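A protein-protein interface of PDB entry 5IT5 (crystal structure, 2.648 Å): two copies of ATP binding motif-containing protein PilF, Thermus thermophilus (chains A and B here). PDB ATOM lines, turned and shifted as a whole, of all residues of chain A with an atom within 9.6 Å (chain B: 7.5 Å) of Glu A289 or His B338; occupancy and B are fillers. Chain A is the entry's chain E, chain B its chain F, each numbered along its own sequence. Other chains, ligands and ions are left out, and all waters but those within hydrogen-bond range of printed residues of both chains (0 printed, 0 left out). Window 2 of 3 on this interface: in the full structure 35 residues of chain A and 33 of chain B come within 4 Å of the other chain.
Hydrophobic or aromatic side chains of chain A that line the printed part of chain B: Leu A294. Along chain A the printed residues that touch a printed residue of chain B span positions 287 to 294. Among the printed residues, no Asp or Glu carboxylate lies within 4 Å of a Lys or Arg side-chain nitrogen of the other chain.
The side-chain carboxylate (OD1) of Asp A287 sits close to the backbone NH (N) of Glu A289, 3.1 Å away. The guanidinium group (NH2) of Arg A292 lies within salt-bridge range of the side-chain carboxylate (OE1) of Glu A289 (3.1 Å). The side-chain carboxylate of Glu A289 is in salt-bridge range of the guanidinium group of Arg A293.
Glu A289 touches His B338. Glu A289 touches Val B341. Ala B342 touches Glu A289 (N to CG, 3.9 Å). CG1 of Val B341 touches OG1 of Thr A290, at 3.9 Å. Phe B258 touches Arg A293. Ala B342 touches Arg A293. CD2 of Leu A294 touches CD2 of Phe B258, at 3.7 Å.
The backbone carbonyl oxygen (O) of Val B341 lies within hydrogen-bond range of the guanidinium group (NE) of Arg A293, at 3.4 Å. The side-chain carboxylate of Asp A287 is in hydrogen-bond range of a ring nitrogen (ND1) of His B338 (2.9 Å).
Of the printed residues of chain B, Asp A287 touches His B338. Of chain B, only His B338 (3.7 Å), Val B341 (3.8 Å) and Ala B342 (3.9 Å) come within 4 Å of Glu A289. Printed residues of chain B within 4 Å of Thr A290: Val B341. Printed residues of chain B within 4 Å of Leu A294: Phe B258 (3.7 Å). Printed residues of chain A within 4 Å of Phe B258: Arg A293 (3.9 Å) and Leu A294 (3.7 Å). Ser B261 touches none of the printed residues of chain A. Asp B333 touches none of the printed residues of chain A. His B338 touches just these residues of chain A: Asp A287 and Glu A289. No residue of chain A comes within 4 Å of Ala B339. Val B341 touches just these residues of chain A: Glu A289 (3.8 Å), Thr A290 (3.9 Å) and Arg A293 (3.4 Å). The nearest residue of chain B that does not touch Glu A289 is Gly B343 (6.1 Å). The nearest residue of chain A that does not touch His B338 is Thr A290 (6.1 Å). The nearest printed residue of chain A that does not touch Phe B258 is Thr A290 (4.3 Å).
No position is printed for both chains.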
ATOM      1  N   LYS A 285      -6.927   0.438  -1.213  1.00  0.00           N
ATOM      2  CA  LYS A 285      -7.405  -0.933  -1.049  1.00  0.00           C
ATOM      3  C   LYS A 285      -7.343  -1.319   0.421  1.00  0.00           C
ATOM      4  O   LYS A 285      -6.258  -1.323   1.017  1.00  0.00           O
ATOM      5  CB  LYS A 285      -6.675  -1.945  -1.917  1.00  0.00           C
ATOM      6  CG  LYS A 285      -7.376  -3.304  -1.849  1.00  0.00           C
ATOM      7  CD  LYS A 285      -7.322  -4.091  -3.148  1.00  0.00           C
ATOM      8  CE  LYS A 285      -8.166  -5.375  -3.071  1.00  0.00           C
ATOM      9  NZ  LYS A 285      -8.238  -6.054  -4.415  1.00  0.00           N
ATOM     10  N   PRO A 286      -8.516  -1.636   0.996  1.00  0.00           N
ATOM     11  CA  PRO A 286      -8.736  -2.014   2.387  1.00  0.00           C
ATOM     12  C   PRO A 286      -8.262  -3.402   2.660  1.00  0.00           C
ATOM     13  O   PRO A 286      -8.314  -4.262   1.791  1.00  0.00           O
ATOM     14  CB  PRO A 286     -10.279  -1.959   2.501  1.00  0.00           C
ATOM     15  CG  PRO A 286     -10.744  -2.226   1.133  1.00  0.00           C
ATOM     16  CD  PRO A 286      -9.753  -1.559   0.233  1.00  0.00           C
ATOM     17  N   ASP A 287      -7.749  -3.589   3.869  1.00  0.00           N
ATOM     18  CA  ASP A 287      -7.434  -4.896   4.367  1.00  0.00           C
ATOM     19  C   ASP A 287      -8.753  -5.663   4.502  1.00  0.00           C
ATOM     20  O   ASP A 287      -9.623  -5.267   5.281  1.00  0.00           O
ATOM     21  CB  ASP A 287      -6.705  -4.758   5.701  1.00  0.00           C
ATOM     22  CG  ASP A 287      -6.041  -6.048   6.155  1.00  0.00           C
ATOM     23  OD1 ASP A 287      -6.452  -7.147   5.698  1.00  0.00           O
ATOM     24  OD2 ASP A 287      -5.120  -5.951   7.003  1.00  0.00           O
ATOM     25  N   PRO A 288      -8.918  -6.743   3.717  1.00  0.00           N
ATOM     26  CA  PRO A 288     -10.098  -7.604   3.832  1.00  0.00           C
ATOM     27  C   PRO A 288     -10.436  -7.931   5.281  1.00  0.00           C
ATOM     28  O   PRO A 288     -11.608  -7.984   5.654  1.00  0.00           O
ATOM     29  CB  PRO A 288      -9.693  -8.868   3.056  1.00  0.00           C
ATOM     30  CG  PRO A 288      -8.250  -8.652   2.619  1.00  0.00           C
ATOM     31  CD  PRO A 288      -8.022  -7.189   2.638  1.00  0.00           C
ATOM     32  N   GLU A 289      -9.410  -8.093   6.102  1.00  0.00           N
ATOM     33  CA  GLU A 289      -9.612  -8.483   7.487  1.00  0.00           C
ATOM     34  C   GLU A 289     -10.315  -7.387   8.289  1.00  0.00           C
ATOM     35  O   GLU A 289     -11.174  -7.677   9.146  1.00  0.00           O
ATOM     36  CB  GLU A 289      -8.273  -8.853   8.118  1.00  0.00           C
ATOM     37  CG  GLU A 289      -8.401  -9.594   9.427  1.00  0.00           C
ATOM     38  CD  GLU A 289      -9.307 -10.813   9.344  1.00  0.00           C
ATOM     39  OE1 GLU A 289      -9.437 -11.416   8.250  1.00  0.00           O
ATOM     40  OE2 GLU A 289      -9.885 -11.164  10.394  1.00  0.00           O
ATOM     41  N   THR A 290      -9.946  -6.138   8.001  1.00  0.00           N
ATOM     42  CA  THR A 290     -10.627  -4.977   8.566  1.00  0.00           C
ATOM     43  C   THR A 290     -12.115  -5.016   8.208  1.00  0.00           C
ATOM     44  O   THR A 290     -12.970  -4.956   9.088  1.00  0.00           O
ATOM     45  CB  THR A 290     -10.021  -3.642   8.058  1.00  0.00           C
ATOM     46  OG1 THR A 290      -8.638  -3.561   8.407  1.00  0.00           O
ATOM     47  CG2 THR A 290     -10.747  -2.462   8.663  1.00  0.00           C
ATOM     48  N   LEU A 291     -12.417  -5.121   6.913  1.00  0.00           N
ATOM     49  CA  LEU A 291     -13.807  -5.160   6.436  1.00  0.00           C
ATOM     50  C   LEU A 291     -14.604  -6.277   7.096  1.00  0.00           C
ATOM     51  O   LEU A 291     -15.715  -6.061   7.578  1.00  0.00           O
ATOM     52  CB  LEU A 291     -13.856  -5.313   4.914  1.00  0.00           C
ATOM     53  CG  LEU A 291     -13.245  -4.108   4.187  1.00  0.00           C
ATOM     54  CD1 LEU A 291     -13.303  -4.280   2.687  1.00  0.00           C
ATOM     55  CD2 LEU A 291     -13.925  -2.798   4.598  1.00  0.00           C
ATOM     56  N   ARG A 292     -14.010  -7.464   7.115  1.00  0.00           N
ATOM     57  CA  ARG A 292     -14.528  -8.598   7.863  1.00  0.00           C
ATOM     58  C   ARG A 292     -14.884  -8.221   9.314  1.00  0.00           C
ATOM     59  O   ARG A 292     -15.987  -8.504   9.776  1.00  0.00           O
ATOM     60  CB  ARG A 292     -13.495  -9.729   7.841  1.00  0.00           C
ATOM     61  CG  ARG A 292     -14.027 -11.128   8.075  1.00  0.00           C
ATOM     62  CD  ARG A 292     -13.582 -12.040   6.944  1.00  0.00           C
ATOM     63  NE  ARG A 292     -12.151 -11.901   6.678  1.00  0.00           N
ATOM     64  CZ  ARG A 292     -11.595 -11.991   5.471  1.00  0.00           C
ATOM     65  NH1 ARG A 292     -12.340 -12.225   4.400  1.00  0.00           N
ATOM     66  NH2 ARG A 292     -10.289 -11.843   5.333  1.00  0.00           N
ATOM     67  N   ARG A 293     -13.967  -7.583  10.035  1.00  0.00           N
ATOM     68  CA  ARG A 293     -14.241  -7.271  11.440  1.00  0.00           C
ATOM     69  C   ARG A 293     -15.353  -6.242  11.566  1.00  0.00           C
ATOM     70  O   ARG A 293     -16.022  -6.174  12.597  1.00  0.00           O
ATOM     71  CB  ARG A 293     -12.987  -6.767  12.161  1.00  0.00           C
ATOM     72  CG  ARG A 293     -11.876  -7.791  12.243  1.00  0.00           C
ATOM     73  CD  ARG A 293     -12.230  -8.946  13.173  1.00  0.00           C
ATOM     74  NE  ARG A 293     -11.362 -10.101  12.952  1.00  0.00           N
ATOM     75  CZ  ARG A 293     -10.994 -10.947  13.911  1.00  0.00           C
ATOM     76  NH1 ARG A 293     -11.418 -10.756  15.154  1.00  0.00           N
ATOM     77  NH2 ARG A 293     -10.208 -11.981  13.636  1.00  0.00           N
ATOM     78  N   LEU A 294     -15.558  -5.455  10.515  1.00  0.00           N
ATOM     79  CA  LEU A 294     -16.578  -4.409  10.539  1.00  0.00           C
ATOM     80  C   LEU A 294     -17.976  -4.947  10.218  1.00  0.00           C
ATOM     81  O   LEU A 294     -18.909  -4.167   9.992  1.00  0.00           O
ATOM     82  CB  LEU A 294     -16.201  -3.289   9.562  1.00  0.00           C
ATOM     83  CG  LEU A 294     -14.973  -2.516  10.037  1.00  0.00           C
ATOM     84  CD1 LEU A 294     -14.496  -1.492   9.030  1.00  0.00           C
ATOM     85  CD2 LEU A 294     -15.290  -1.844  11.362  1.00  0.00           C
ATOM     86  N   GLY A 295     -18.103  -6.276  10.194  1.00  0.00           N
ATOM     87  CA  GLY A 295     -19.361  -6.949   9.928  1.00  0.00           C
ATOM     88  C   GLY A 295     -19.785  -6.941   8.463  1.00  0.00           C
ATOM     89  O   GLY A 295     -20.898  -7.389   8.112  1.00  0.00           O
ATOM     90  N   LEU A 296     -18.917  -6.418   7.598  1.00  0.00           N
ATOM     91  CA  LEU A 296     -19.238  -6.393   6.172  1.00  0.00           C
ATOM     92  C   LEU A 296     -19.237  -7.817   5.685  1.00  0.00           C
ATOM     93  O   LEU A 296     -18.313  -8.571   5.977  1.00  0.00           O
ATOM     94  CB  LEU A 296     -18.252  -5.552   5.368  1.00  0.00           C
ATOM     95  CG  LEU A 296     -18.385  -5.611   3.842  1.00  0.00           C
ATOM     96  CD1 LEU A 296     -19.706  -4.985   3.390  1.00  0.00           C
ATOM     97  CD2 LEU A 296     -17.186  -4.937   3.144  1.00  0.00           C
ATOM     98  N   GLU A 298     -18.704 -11.137   3.795  1.00  0.00           N
ATOM     99  CA  GLU A 298     -17.922 -11.827   2.774  1.00  0.00           C
ATOM    100  C   GLU A 298     -18.906 -12.023   1.644  1.00  0.00           C
ATOM    101  O   GLU A 298     -20.100 -12.229   1.911  1.00  0.00           O
ATOM    102  CB  GLU A 298     -17.368 -13.169   3.260  1.00  0.00           C
ATOM    103  CG  GLU A 298     -16.365 -13.058   4.391  1.00  0.00           C
ATOM    104  CD  GLU A 298     -15.093 -13.855   4.128  1.00  0.00           C
ATOM    105  OE1 GLU A 298     -14.406 -13.570   3.113  1.00  0.00           O
ATOM    106  OE2 GLU A 298     -14.781 -14.757   4.940  1.00  0.00           O
ATOM    107  N   ILE A 301     -16.884  -8.343  -0.019  1.00  0.00           N
ATOM    108  CA  ILE A 301     -15.547  -7.912   0.337  1.00  0.00           C
ATOM    109  C   ILE A 301     -14.585  -7.748  -0.854  1.00  0.00           C
ATOM    110  O   ILE A 301     -13.507  -7.192  -0.700  1.00  0.00           O
ATOM    111  CB  ILE A 301     -14.996  -8.916   1.354  1.00  0.00           C
ATOM    112  CG1 ILE A 301     -13.654  -8.483   1.934  1.00  0.00           C
ATOM    113  CG2 ILE A 301     -14.972 -10.312   0.739  1.00  0.00           C
ATOM    114  CD1 ILE A 301     -13.272  -9.317   3.120  1.00  0.00           C
ATOM    115  N   ALA A 304     -14.760  -3.836  -2.652  1.00  0.00           N
ATOM    116  CA  ALA A 304     -13.677  -3.444  -1.763  1.00  0.00           C
ATOM    117  C   ALA A 304     -12.964  -2.157  -2.068  1.00  0.00           C
ATOM    118  O   ALA A 304     -11.738  -2.156  -2.062  1.00  0.00           O
ATOM    119  CB  ALA A 304     -12.623  -4.561  -1.724  1.00  0.00           C
ATOM    120  N   LEU A 376     -12.817   5.842   5.833  1.00  0.00           N
ATOM    121  CA  LEU A 376     -13.182   4.905   6.887  1.00  0.00           C
ATOM    122  C   LEU A 376     -12.773   5.437   8.263  1.00  0.00           C
ATOM    123  O   LEU A 376     -13.407   5.108   9.277  1.00  0.00           O
ATOM    124  CB  LEU A 376     -12.549   3.540   6.631  1.00  0.00           C
ATOM    125  CG  LEU A 376     -12.991   2.435   7.594  1.00  0.00           C
ATOM    126  CD1 LEU A 376     -14.466   2.276   7.514  1.00  0.00           C
ATOM    127  CD2 LEU A 376     -12.330   1.130   7.235  1.00  0.00           C
ATOM    128  N   PHE B 258      -9.702  -2.965  14.982  1.00  0.00           N
ATOM    129  CA  PHE B 258      -9.751  -2.214  13.726  1.00  0.00           C
ATOM    130  C   PHE B 258      -9.543  -0.733  14.026  1.00  0.00           C
ATOM    131  O   PHE B 258      -9.036  -0.011  13.187  1.00  0.00           O
ATOM    132  CB  PHE B 258     -11.049  -2.447  12.912  1.00  0.00           C
ATOM    133  CG  PHE B 258     -12.334  -2.274  13.690  1.00  0.00           C
ATOM    134  CD1 PHE B 258     -12.781  -1.018  14.071  1.00  0.00           C
ATOM    135  CD2 PHE B 258     -13.126  -3.386  13.998  1.00  0.00           C
ATOM    136  CE1 PHE B 258     -13.975  -0.878  14.781  1.00  0.00           C
ATOM    137  CE2 PHE B 258     -14.310  -3.252  14.700  1.00  0.00           C
ATOM    138  CZ  PHE B 258     -14.737  -2.000  15.091  1.00  0.00           C
ATOM    139  N   SER B 261      -5.654  -0.543  14.777  1.00  0.00           N
ATOM    140  CA  SER B 261      -4.894  -0.664  13.534  1.00  0.00           C
ATOM    141  C   SER B 261      -4.879   0.647  12.721  1.00  0.00           C
ATOM    142  O   SER B 261      -3.853   1.020  12.117  1.00  0.00           O
ATOM    143  CB  SER B 261      -5.466  -1.802  12.698  1.00  0.00           C
ATOM    144  OG  SER B 261      -4.950  -1.751  11.396  1.00  0.00           O
ATOM    145  N   VAL B 332       4.662   0.907  13.559  1.00  0.00           N
ATOM    146  CA  VAL B 332       3.592   0.204  12.866  1.00  0.00           C
ATOM    147  C   VAL B 332       3.655   0.393  11.336  1.00  0.00           C
ATOM    148  O   VAL B 332       3.721   1.519  10.839  1.00  0.00           O
ATOM    149  CB  VAL B 332       2.230   0.654  13.403  1.00  0.00           C
ATOM    150  CG1 VAL B 332       1.115   0.066  12.578  1.00  0.00           C
ATOM    151  CG2 VAL B 332       2.096   0.231  14.860  1.00  0.00           C
ATOM    152  N   ASP B 333       3.660  -0.726  10.610  1.00  0.00           N
ATOM    153  CA  ASP B 333       3.532  -0.727   9.152  1.00  0.00           C
ATOM    154  C   ASP B 333       2.340  -1.607   8.717  1.00  0.00           C
ATOM    155  O   ASP B 333       1.512  -1.983   9.556  1.00  0.00           O
ATOM    156  CB  ASP B 333       4.829  -1.192   8.496  1.00  0.00           C
ATOM    157  CG  ASP B 333       5.273  -2.571   8.955  1.00  0.00           C
ATOM    158  OD1 ASP B 333       4.444  -3.356   9.465  1.00  0.00           O
ATOM    159  OD2 ASP B 333       6.472  -2.881   8.796  1.00  0.00           O
ATOM    160  N   ASP B 334       2.243  -1.935   7.428  1.00  0.00           N
ATOM    161  CA  ASP B 334       1.058  -2.637   6.924  1.00  0.00           C
ATOM    162  C   ASP B 334       1.011  -4.063   7.494  1.00  0.00           C
ATOM    163  O   ASP B 334      -0.044  -4.558   7.900  1.00  0.00           O
ATOM    164  CB  ASP B 334       1.031  -2.663   5.389  1.00  0.00           C
ATOM    165  CG  ASP B 334       0.716  -1.293   4.762  1.00  0.00           C
ATOM    166  OD1 ASP B 334      -0.014  -0.474   5.369  1.00  0.00           O
ATOM    167  OD2 ASP B 334       1.189  -1.042   3.629  1.00  0.00           O
ATOM    168  N   GLU B 335       2.162  -4.714   7.562  1.00  0.00           N
ATOM    169  CA  GLU B 335       2.219  -6.065   8.117  1.00  0.00           C
ATOM    170  C   GLU B 335       1.848  -6.126   9.616  1.00  0.00           C
ATOM    171  O   GLU B 335       1.094  -7.007  10.037  1.00  0.00           O
ATOM    172  CB  GLU B 335       3.603  -6.665   7.888  1.00  0.00           C
ATOM    173  CG  GLU B 335       3.697  -8.122   8.281  1.00  0.00           C
ATOM    174  CD  GLU B 335       5.039  -8.734   7.906  1.00  0.00           C
ATOM    175  OE1 GLU B 335       5.895  -7.991   7.347  1.00  0.00           O
ATOM    176  OE2 GLU B 335       5.232  -9.951   8.165  1.00  0.00           O
ATOM    177  N   ILE B 336       2.363  -5.189  10.410  1.00  0.00           N
ATOM    178  CA  ILE B 336       1.938  -5.051  11.805  1.00  0.00           C
ATOM    179  C   ILE B 336       0.444  -4.737  11.964  1.00  0.00           C
ATOM    180  O   ILE B 336      -0.240  -5.380  12.771  1.00  0.00           O
ATOM    181  CB  ILE B 336       2.712  -3.941  12.531  1.00  0.00           C
ATOM    182  CG1 ILE B 336       4.221  -4.200  12.474  1.00  0.00           C
ATOM    183  CG2 ILE B 336       2.254  -3.858  13.972  1.00  0.00           C
ATOM    184  CD1 ILE B 336       4.663  -5.378  13.303  1.00  0.00           C
ATOM    185  N   ARG B 337      -0.069  -3.758  11.212  1.00  0.00           N
ATOM    186  CA  ARG B 337      -1.453  -3.322  11.434  1.00  0.00           C
ATOM    187  C   ARG B 337      -2.415  -4.413  11.003  1.00  0.00           C
ATOM    188  O   ARG B 337      -3.525  -4.508  11.525  1.00  0.00           O
ATOM    189  CB  ARG B 337      -1.777  -1.999  10.724  1.00  0.00           C
ATOM    190  CG  ARG B 337      -1.724  -2.068   9.256  1.00  0.00           C
ATOM    191  CD  ARG B 337      -2.007  -0.704   8.664  1.00  0.00           C
ATOM    192  NE  ARG B 337      -1.247   0.371   9.310  1.00  0.00           N
ATOM    193  CZ  ARG B 337      -0.270   1.070   8.725  1.00  0.00           C
ATOM    194  NH1 ARG B 337       0.091   0.812   7.471  1.00  0.00           N
ATOM    195  NH2 ARG B 337       0.345   2.035   9.393  1.00  0.00           N
ATOM    196  N   HIS B 338      -1.976  -5.263  10.084  1.00  0.00           N
ATOM    197  CA  HIS B 338      -2.760  -6.430   9.726  1.00  0.00           C
ATOM    198  C   HIS B 338      -2.789  -7.447  10.871  1.00  0.00           C
ATOM    199  O   HIS B 338      -3.818  -8.085  11.116  1.00  0.00           O
ATOM    200  CB  HIS B 338      -2.216  -7.083   8.458  1.00  0.00           C
ATOM    201  CG  HIS B 338      -2.940  -8.335   8.075  1.00  0.00           C
ATOM    202  ND1 HIS B 338      -4.306  -8.479   8.213  1.00  0.00           N
ATOM    203  CD2 HIS B 338      -2.486  -9.512   7.585  1.00  0.00           C
ATOM    204  CE1 HIS B 338      -4.663  -9.683   7.807  1.00  0.00           C
ATOM    205  NE2 HIS B 338      -3.576 -10.334   7.426  1.00  0.00           N
ATOM    206  N   ALA B 339      -1.672  -7.598  11.578  1.00  0.00           N
ATOM    207  CA  ALA B 339      -1.632  -8.546  12.684  1.00  0.00           C
ATOM    208  C   ALA B 339      -2.526  -8.090  13.841  1.00  0.00           C
ATOM    209  O   ALA B 339      -2.941  -8.894  14.675  1.00  0.00           O
ATOM    210  CB  ALA B 339      -0.226  -8.740  13.161  1.00  0.00           C
ATOM    211  N   ILE B 340      -2.819  -6.795  13.899  1.00  0.00           N
ATOM    212  CA  ILE B 340      -3.679  -6.295  14.947  1.00  0.00           C
ATOM    213  C   ILE B 340      -5.106  -6.754  14.694  1.00  0.00           C
ATOM    214  O   ILE B 340      -5.727  -7.307  15.593  1.00  0.00           O
ATOM    215  CB  ILE B 340      -3.663  -4.768  15.042  1.00  0.00           C
ATOM    216  CG1 ILE B 340      -2.263  -4.205  14.787  1.00  0.00           C
ATOM    217  CG2 ILE B 340      -4.198  -4.323  16.386  1.00  0.00           C
ATOM    218  CD1 ILE B 340      -1.294  -4.502  15.847  1.00  0.00           C
ATOM    219  N   VAL B 341      -5.625  -6.522  13.481  1.00  0.00           N
ATOM    220  CA  VAL B 341      -7.028  -6.865  13.179  1.00  0.00           C
ATOM    221  C   VAL B 341      -7.175  -8.362  13.092  1.00  0.00           C
ATOM    222  O   VAL B 341      -8.193  -8.917  13.501  1.00  0.00           O
ATOM    223  CB  VAL B 341      -7.554  -6.239  11.864  1.00  0.00           C
ATOM    224  CG1 VAL B 341      -7.822  -4.768  12.046  1.00  0.00           C
ATOM    225  CG2 VAL B 341      -6.586  -6.469  10.724  1.00  0.00           C
ATOM    226  N   ALA B 342      -6.139  -9.010  12.567  1.00  0.00           N
ATOM    227  CA  ALA B 342      -6.054 -10.460  12.539  1.00  0.00           C
ATOM    228  C   ALA B 342      -6.197 -11.023  13.936  1.00  0.00           C
ATOM    229  O   ALA B 342      -6.651 -12.148  14.103  1.00  0.00           O
ATOM    230  CB  ALA B 342      -4.743 -10.910  11.931  1.00  0.00           C
ATOM    231  N   GLY B 343      -5.793 -10.250  14.938  1.00  0.00           N
ATOM    232  CA  GLY B 343      -6.008 -10.633  16.321  1.00  0.00           C
ATOM    233  C   GLY B 343      -4.892 -11.466  16.920  1.00  0.00           C
ATOM    234  O   GLY B 343      -5.110 -12.268  17.830  1.00  0.00           O
ATOM    235  N   LYS B 344      -3.682 -11.273  16.418  1.00  0.00           N
ATOM    236  CA  LYS B 344      -2.539 -12.008  16.934  1.00  0.00           C
ATOM    237  C   LYS B 344      -2.145 -11.454  18.307  1.00  0.00           C
ATOM    238  O   LYS B 344      -2.536 -10.334  18.659  1.00  0.00           O
ATOM    239  CB  LYS B 344      -1.390 -11.951  15.937  1.00  0.00           C
ATOM    240  CG  LYS B 344      -1.770 -12.489  14.559  1.00  0.00           C
ATOM    241  CD  LYS B 344      -0.512 -12.908  13.847  1.00  0.00           C
ATOM    242  CE  LYS B 344      -0.760 -13.532  12.490  1.00  0.00           C
ATOM    243  NZ  LYS B 344       0.568 -13.806  11.842  1.00  0.00           N
ATOM    244  N   ILE B 349       2.974 -10.569  17.624  1.00  0.00           N
ATOM    245  CA  ILE B 349       3.222  -9.253  17.031  1.00  0.00           C
ATOM    246  C   ILE B 349       4.664  -8.818  17.251  1.00  0.00           C
ATOM    247  O   ILE B 349       5.275  -8.191  16.381  1.00  0.00           O
ATOM    248  CB  ILE B 349       2.277  -8.172  17.602  1.00  0.00           C
ATOM    249  CG1 ILE B 349       0.852  -8.366  17.084  1.00  0.00           C
ATOM    250  CG2 ILE B 349       2.703  -6.806  17.160  1.00  0.00           C
ATOM    251  CD1 ILE B 349      -0.151  -7.404  17.714  1.00  0.00           C
ATOM    252  N   ILE B 352       7.058 -10.431  14.836  1.00  0.00           N
ATOM    253  CA  ILE B 352       6.996  -9.802  13.518  1.00  0.00           C
ATOM    254  C   ILE B 352       7.855  -8.548  13.509  1.00  0.00           C
ATOM    255  O   ILE B 352       8.661  -8.324  12.599  1.00  0.00           O
ATOM    256  CB  ILE B 352       5.531  -9.441  13.120  1.00  0.00           C
ATOM    257  CG1 ILE B 352       4.675 -10.698  13.024  1.00  0.00           C
ATOM    258  CG2 ILE B 352       5.477  -8.733  11.797  1.00  0.00           C
ATOM    259  CD1 ILE B 352       3.201 -10.421  12.775  1.00  0.00           C
